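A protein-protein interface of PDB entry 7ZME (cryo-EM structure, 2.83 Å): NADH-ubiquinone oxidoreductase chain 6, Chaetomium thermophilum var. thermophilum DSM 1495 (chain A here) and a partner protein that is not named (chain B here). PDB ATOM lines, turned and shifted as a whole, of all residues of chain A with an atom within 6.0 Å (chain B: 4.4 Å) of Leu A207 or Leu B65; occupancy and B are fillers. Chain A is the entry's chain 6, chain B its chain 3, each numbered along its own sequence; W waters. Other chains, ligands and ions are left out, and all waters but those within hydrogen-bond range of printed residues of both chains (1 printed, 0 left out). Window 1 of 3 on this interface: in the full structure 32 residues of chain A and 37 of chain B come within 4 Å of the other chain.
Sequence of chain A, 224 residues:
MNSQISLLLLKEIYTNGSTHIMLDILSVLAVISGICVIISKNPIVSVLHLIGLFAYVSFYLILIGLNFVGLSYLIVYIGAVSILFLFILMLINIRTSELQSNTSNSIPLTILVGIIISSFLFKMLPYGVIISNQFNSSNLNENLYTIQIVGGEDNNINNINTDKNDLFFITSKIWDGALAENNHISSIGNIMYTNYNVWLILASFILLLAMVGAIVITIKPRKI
The side-chain carboxylate (OE1) of Glu B69 lies close to the side-chain sulfur (SD) of Met A211 (3.5 Å).
Among the printed residues, pairs that only touch across the chains: Leu A207 with Glu B69, Met A211 with Leu B65, Ala A210 with Leu B65, Leu A207 with Leu B65, Ser A204 with Ile B98 and Leu A207 with Leu B68.
Of the printed residues of chain B, Leu A207 touches Leu B65, Leu B68 and Glu B69. Printed residues of chain B within 4 Å of Ala A210: Leu B65. Of the printed residues of chain B, Met A211 touches Leu B65 (3.5 Å) and Glu B69 (3.5 Å). Asp B67 touches none of the printed residues of chain A. Printed residues of chain A within 4 Å of Ile B98: Ser A204.
Of the 12 printed residues of chain A, 4 touch a printed residue of chain B. Hydrophobic or aromatic side chains of chain A that line the printed part of chain B: Leu A207, Ala A210 and Met A211. Among the printed residues, 7 pairs touch across the chains.
Water W1 bridges O of Val B62 (2.7 Å) and SD of Met A211 (3.6 Å).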
ATOM      1  N   LEU A 202     -31.534   9.157   4.517  1.00  0.00           N
ATOM      2  CA  LEU A 202     -30.550   9.913   5.283  1.00  0.00           C
ATOM      3  C   LEU A 202     -29.412  10.402   4.401  1.00  0.00           C
ATOM      4  O   LEU A 202     -28.970  11.548   4.528  1.00  0.00           O
ATOM      5  CB  LEU A 202     -30.012   9.069   6.441  1.00  0.00           C
ATOM      6  CG  LEU A 202     -30.797   8.996   7.756  1.00  0.00           C
ATOM      7  CD1 LEU A 202     -30.849  10.363   8.401  1.00  0.00           C
ATOM      8  CD2 LEU A 202     -32.209   8.473   7.562  1.00  0.00           C
ATOM      9  N   ALA A 203     -28.921   9.550   3.499  1.00  0.00           N
ATOM     10  CA  ALA A 203     -27.843   9.964   2.608  1.00  0.00           C
ATOM     11  C   ALA A 203     -28.281  11.108   1.706  1.00  0.00           C
ATOM     12  O   ALA A 203     -27.501  12.024   1.429  1.00  0.00           O
ATOM     13  CB  ALA A 203     -27.361   8.781   1.776  1.00  0.00           C
ATOM     14  N   SER A 204     -29.530  11.075   1.240  1.00  0.00           N
ATOM     15  CA  SER A 204     -30.044  12.143   0.396  1.00  0.00           C
ATOM     16  C   SER A 204     -30.227  13.448   1.155  1.00  0.00           C
ATOM     17  O   SER A 204     -30.264  14.511   0.528  1.00  0.00           O
ATOM     18  CB  SER A 204     -31.370  11.720  -0.234  1.00  0.00           C
ATOM     19  OG  SER A 204     -32.427  11.827   0.697  1.00  0.00           O
ATOM     20  N   PHE A 205     -30.347  13.400   2.480  1.00  0.00           N
ATOM     21  CA  PHE A 205     -30.448  14.621   3.268  1.00  0.00           C
ATOM     22  C   PHE A 205     -29.085  15.192   3.621  1.00  0.00           C
ATOM     23  O   PHE A 205     -28.954  16.411   3.777  1.00  0.00           O
ATOM     24  CB  PHE A 205     -31.263  14.372   4.540  1.00  0.00           C
ATOM     25  CG  PHE A 205     -32.705  14.760   4.405  1.00  0.00           C
ATOM     26  CD1 PHE A 205     -33.612  13.905   3.810  1.00  0.00           C
ATOM     27  CD2 PHE A 205     -33.146  15.999   4.835  1.00  0.00           C
ATOM     28  CE1 PHE A 205     -34.935  14.268   3.669  1.00  0.00           C
ATOM     29  CE2 PHE A 205     -34.466  16.368   4.695  1.00  0.00           C
ATOM     30  CZ  PHE A 205     -35.362  15.501   4.111  1.00  0.00           C
ATOM     31  N   ILE A 206     -28.062  14.356   3.671  1.00  0.00           N
ATOM     32  CA  ILE A 206     -26.682  14.885   3.858  1.00  0.00           C
ATOM     33  C   ILE A 206     -26.340  15.626   2.563  1.00  0.00           C
ATOM     34  O   ILE A 206     -25.863  16.767   2.655  1.00  0.00           O
ATOM     35  CB  ILE A 206     -25.699  13.741   4.181  1.00  0.00           C
ATOM     36  CG1 ILE A 206     -26.140  12.974   5.429  1.00  0.00           C
ATOM     37  CG2 ILE A 206     -24.278  14.257   4.311  1.00  0.00           C
ATOM     38  CD1 ILE A 206     -25.430  11.659   5.627  1.00  0.00           C
ATOM     39  N   LEU A 207     -26.588  15.008   1.412  1.00  0.00           N
ATOM     40  CA  LEU A 207     -26.304  15.629   0.095  1.00  0.00           C
ATOM     41  C   LEU A 207     -27.082  16.935  -0.086  1.00  0.00           C
ATOM     42  O   LEU A 207     -26.488  17.871  -0.616  1.00  0.00           O
ATOM     43  CB  LEU A 207     -26.763  14.632  -0.964  1.00  0.00           C
ATOM     44  CG  LEU A 207     -25.902  13.393  -1.156  1.00  0.00           C
ATOM     45  CD1 LEU A 207     -26.754  12.273  -1.714  1.00  0.00           C
ATOM     46  CD2 LEU A 207     -24.722  13.691  -2.070  1.00  0.00           C
ATOM     47  N   LEU A 208     -28.348  16.989   0.326  1.00  0.00           N
ATOM     48  CA  LEU A 208     -29.178  18.215   0.237  1.00  0.00           C
ATOM     49  C   LEU A 208     -28.581  19.336   1.088  1.00  0.00           C
ATOM     50  O   LEU A 208     -28.505  20.467   0.598  1.00  0.00           O
ATOM     51  CB  LEU A 208     -30.564  17.865   0.786  1.00  0.00           C
ATOM     52  CG  LEU A 208     -31.674  18.874   0.521  1.00  0.00           C
ATOM     53  CD1 LEU A 208     -31.980  18.936  -0.961  1.00  0.00           C
ATOM     54  CD2 LEU A 208     -32.920  18.495   1.299  1.00  0.00           C
ATOM     55  N   LEU A 209     -28.187  19.027   2.317  1.00  0.00           N
ATOM     56  CA  LEU A 209     -27.594  20.041   3.213  1.00  0.00           C
ATOM     57  C   LEU A 209     -26.283  20.515   2.587  1.00  0.00           C
ATOM     58  O   LEU A 209     -26.008  21.715   2.643  1.00  0.00           O
ATOM     59  CB  LEU A 209     -27.386  19.408   4.592  1.00  0.00           C
ATOM     60  CG  LEU A 209     -26.496  20.165   5.573  1.00  0.00           C
ATOM     61  CD1 LEU A 209     -27.198  21.405   6.101  1.00  0.00           C
ATOM     62  CD2 LEU A 209     -26.092  19.258   6.718  1.00  0.00           C
ATOM     63  N   ALA A 210     -25.514  19.607   1.989  1.00  0.00           N
ATOM     64  CA  ALA A 210     -24.256  19.999   1.322  1.00  0.00           C
ATOM     65  C   ALA A 210     -24.535  20.890   0.109  1.00  0.00           C
ATOM     66  O   ALA A 210     -23.809  21.866  -0.082  1.00  0.00           O
ATOM     67  CB  ALA A 210     -23.467  18.782   0.956  1.00  0.00           C
ATOM     68  N   MET A 211     -25.556  20.564  -0.676  1.00  0.00           N
ATOM     69  CA  MET A 211     -25.920  21.370  -1.869  1.00  0.00           C
ATOM     70  C   MET A 211     -26.368  22.768  -1.444  1.00  0.00           C
ATOM     71  O   MET A 211     -25.998  23.729  -2.125  1.00  0.00           O
ATOM     72  CB  MET A 211     -27.048  20.697  -2.654  1.00  0.00           C
ATOM     73  CG  MET A 211     -26.724  19.311  -3.149  1.00  0.00           C
ATOM     74  SD  MET A 211     -28.075  18.676  -4.170  1.00  0.00           S
ATOM     75  CE  MET A 211     -28.101  19.908  -5.469  1.00  0.00           C
ATOM     76  N   VAL A 212     -27.130  22.869  -0.358  1.00  0.00           N
ATOM     77  CA  VAL A 212     -27.673  24.180   0.108  1.00  0.00           C
ATOM     78  C   VAL A 212     -26.588  24.941   0.871  1.00  0.00           C
ATOM     79  O   VAL A 212     -26.426  26.137   0.600  1.00  0.00           O
ATOM     80  CB  VAL A 212     -28.945  23.979   0.957  1.00  0.00           C
ATOM     81  CG1 VAL A 212     -29.389  25.257   1.654  1.00  0.00           C
ATOM     82  CG2 VAL A 212     -30.077  23.387   0.137  1.00  0.00           C
ATOM     83  N   ALA A 214     -23.094  24.551   0.924  1.00  0.00           N
ATOM     84  CA  ALA A 214     -21.844  24.944   0.235  1.00  0.00           C
ATOM     85  C   ALA A 214     -22.133  26.194  -0.594  1.00  0.00           C
ATOM     86  O   ALA A 214     -21.281  27.085  -0.626  1.00  0.00           O
ATOM     87  CB  ALA A 214     -21.286  23.809  -0.592  1.00  0.00           C
ATOM     88  N   LEU B  61     -18.460  22.571  -7.040  1.00  0.00           N
ATOM     89  CA  LEU B  61     -19.004  22.083  -5.750  1.00  0.00           C
ATOM     90  C   LEU B  61     -20.278  21.270  -6.001  1.00  0.00           C
ATOM     91  O   LEU B  61     -20.397  20.193  -5.405  1.00  0.00           O
ATOM     92  CB  LEU B  61     -19.260  23.284  -4.837  1.00  0.00           C
ATOM     93  CG  LEU B  61     -18.020  23.960  -4.259  1.00  0.00           C
ATOM     94  CD1 LEU B  61     -18.388  25.252  -3.549  1.00  0.00           C
ATOM     95  CD2 LEU B  61     -17.292  23.023  -3.312  1.00  0.00           C
ATOM     96  N   VAL B  62     -21.202  21.778  -6.820  1.00  0.00           N
ATOM     97  CA  VAL B  62     -22.493  21.091  -7.128  1.00  0.00           C
ATOM     98  C   VAL B  62     -22.264  19.807  -7.933  1.00  0.00           C
ATOM     99  O   VAL B  62     -22.985  18.835  -7.687  1.00  0.00           O
ATOM    100  CB  VAL B  62     -23.497  22.046  -7.801  1.00  0.00           C
ATOM    101  CG1 VAL B  62     -23.920  23.171  -6.872  1.00  0.00           C
ATOM    102  CG2 VAL B  62     -22.967  22.598  -9.114  1.00  0.00           C
ATOM    103  N   PHE B  63     -21.303  19.808  -8.858  1.00  0.00           N
ATOM    104  CA  PHE B  63     -21.019  18.635  -9.725  1.00  0.00           C
ATOM    105  C   PHE B  63     -20.630  17.439  -8.863  1.00  0.00           C
ATOM    106  O   PHE B  63     -21.046  16.329  -9.195  1.00  0.00           O
ATOM    107  CB  PHE B  63     -19.913  18.998 -10.721  1.00  0.00           C
ATOM    108  CG  PHE B  63     -18.953  17.899 -11.103  1.00  0.00           C
ATOM    109  CD1 PHE B  63     -19.226  17.057 -12.163  1.00  0.00           C
ATOM    110  CD2 PHE B  63     -17.755  17.734 -10.431  1.00  0.00           C
ATOM    111  CE1 PHE B  63     -18.352  16.044 -12.514  1.00  0.00           C
ATOM    112  CE2 PHE B  63     -16.881  16.719 -10.780  1.00  0.00           C
ATOM    113  CZ  PHE B  63     -17.179  15.878 -11.823  1.00  0.00           C
ATOM    114  N   LEU B  64     -19.863  17.673  -7.801  1.00  0.00           N
ATOM    115  CA  LEU B  64     -19.397  16.572  -6.929  1.00  0.00           C
ATOM    116  C   LEU B  64     -20.597  15.871  -6.301  1.00  0.00           C
ATOM    117  O   LEU B  64     -20.644  14.637  -6.359  1.00  0.00           O
ATOM    118  CB  LEU B  64     -18.545  17.196  -5.820  1.00  0.00           C
ATOM    119  CG  LEU B  64     -17.197  17.765  -6.247  1.00  0.00           C
ATOM    120  CD1 LEU B  64     -16.417  18.244  -5.035  1.00  0.00           C
ATOM    121  CD2 LEU B  64     -16.404  16.724  -7.013  1.00  0.00           C
ATOM    122  N   LEU B  65     -21.537  16.637  -5.762  1.00  0.00           N
ATOM    123  CA  LEU B  65     -22.723  16.064  -5.090  1.00  0.00           C
ATOM    124  C   LEU B  65     -23.641  15.353  -6.084  1.00  0.00           C
ATOM    125  O   LEU B  65     -24.114  14.264  -5.758  1.00  0.00           O
ATOM    126  CB  LEU B  65     -23.441  17.207  -4.367  1.00  0.00           C
ATOM    127  CG  LEU B  65     -22.548  18.055  -3.464  1.00  0.00           C
ATOM    128  CD1 LEU B  65     -23.236  19.352  -3.077  1.00  0.00           C
ATOM    129  CD2 LEU B  65     -22.124  17.274  -2.231  1.00  0.00           C
ATOM    130  N   LEU B  66     -23.902  15.957  -7.237  1.00  0.00           N
ATOM    131  CA  LEU B  66     -24.796  15.356  -8.256  1.00  0.00           C
ATOM    132  C   LEU B  66     -24.156  14.106  -8.852  1.00  0.00           C
ATOM    133  O   LEU B  66     -24.896  13.191  -9.231  1.00  0.00           O
ATOM    134  CB  LEU B  66     -25.162  16.413  -9.296  1.00  0.00           C
ATOM    135  CG  LEU B  66     -26.553  17.024  -9.136  1.00  0.00           C
ATOM    136  CD1 LEU B  66     -26.696  18.284  -9.973  1.00  0.00           C
ATOM    137  CD2 LEU B  66     -27.628  16.012  -9.500  1.00  0.00           C
ATOM    138  N   ASP B  67     -22.830  14.091  -8.951  1.00  0.00           N
ATOM    139  CA  ASP B  67     -22.100  12.898  -9.437  1.00  0.00           C
ATOM    140  C   ASP B  67     -22.388  11.773  -8.442  1.00  0.00           C
ATOM    141  O   ASP B  67     -22.537  10.625  -8.871  1.00  0.00           O
ATOM    142  CB  ASP B  67     -20.610  13.219  -9.568  1.00  0.00           C
ATOM    143  CG  ASP B  67     -19.796  12.305 -10.469  1.00  0.00           C
ATOM    144  OD1 ASP B  67     -20.324  11.267 -10.894  1.00  0.00           O
ATOM    145  OD2 ASP B  67     -18.629  12.646 -10.737  1.00  0.00           O
ATOM    146  N   LEU B  68     -22.504  12.115  -7.164  1.00  0.00           N
ATOM    147  CA  LEU B  68     -22.720  11.077  -6.126  1.00  0.00           C
ATOM    148  C   LEU B  68     -24.153  10.590  -6.286  1.00  0.00           C
ATOM    149  O   LEU B  68     -24.387   9.381  -6.145  1.00  0.00           O
ATOM    150  CB  LEU B  68     -22.492  11.696  -4.749  1.00  0.00           C
ATOM    151  CG  LEU B  68     -21.045  12.064  -4.429  1.00  0.00           C
ATOM    152  CD1 LEU B  68     -20.971  12.971  -3.213  1.00  0.00           C
ATOM    153  CD2 LEU B  68     -20.203  10.818  -4.221  1.00  0.00           C
ATOM    154  N   GLU B  69     -25.073  11.514  -6.559  1.00  0.00           N
ATOM    155  CA  GLU B  69     -26.519  11.208  -6.704  1.00  0.00           C
ATOM    156  C   GLU B  69     -26.843  10.305  -7.901  1.00  0.00           C
ATOM    157  O   GLU B  69     -27.728   9.451  -7.740  1.00  0.00           O
ATOM    158  CB  GLU B  69     -27.281  12.531  -6.668  1.00  0.00           C
ATOM    159  CG  GLU B  69     -27.205  13.190  -5.305  1.00  0.00           C
ATOM    160  CD  GLU B  69     -27.286  14.705  -5.267  1.00  0.00           C
ATOM    161  OE1 GLU B  69     -27.081  15.279  -4.180  1.00  0.00           O
ATOM    162  OE2 GLU B  69     -27.551  15.305  -6.317  1.00  0.00           O
ATOM    163  N   ILE B  98     -33.518  15.147  -4.031  1.00  0.00           N
ATOM    164  CA  ILE B  98     -32.323  15.676  -4.754  1.00  0.00           C
ATOM    165  C   ILE B  98     -32.739  16.810  -5.691  1.00  0.00           C
ATOM    166  O   ILE B  98     -32.017  17.815  -5.752  1.00  0.00           O
ATOM    167  CB  ILE B  98     -31.590  14.529  -5.469  1.00  0.00           C
ATOM    168  CG1 ILE B  98     -30.887  13.598  -4.478  1.00  0.00           C
ATOM    169  CG2 ILE B  98     -30.650  15.047  -6.543  1.00  0.00           C
ATOM    170  CD1 ILE B  98     -30.337  14.293  -3.256  1.00  0.00           C
HETATM  171  O   HOH W   1     -25.131  19.332  -6.178  1.00  0.00           O
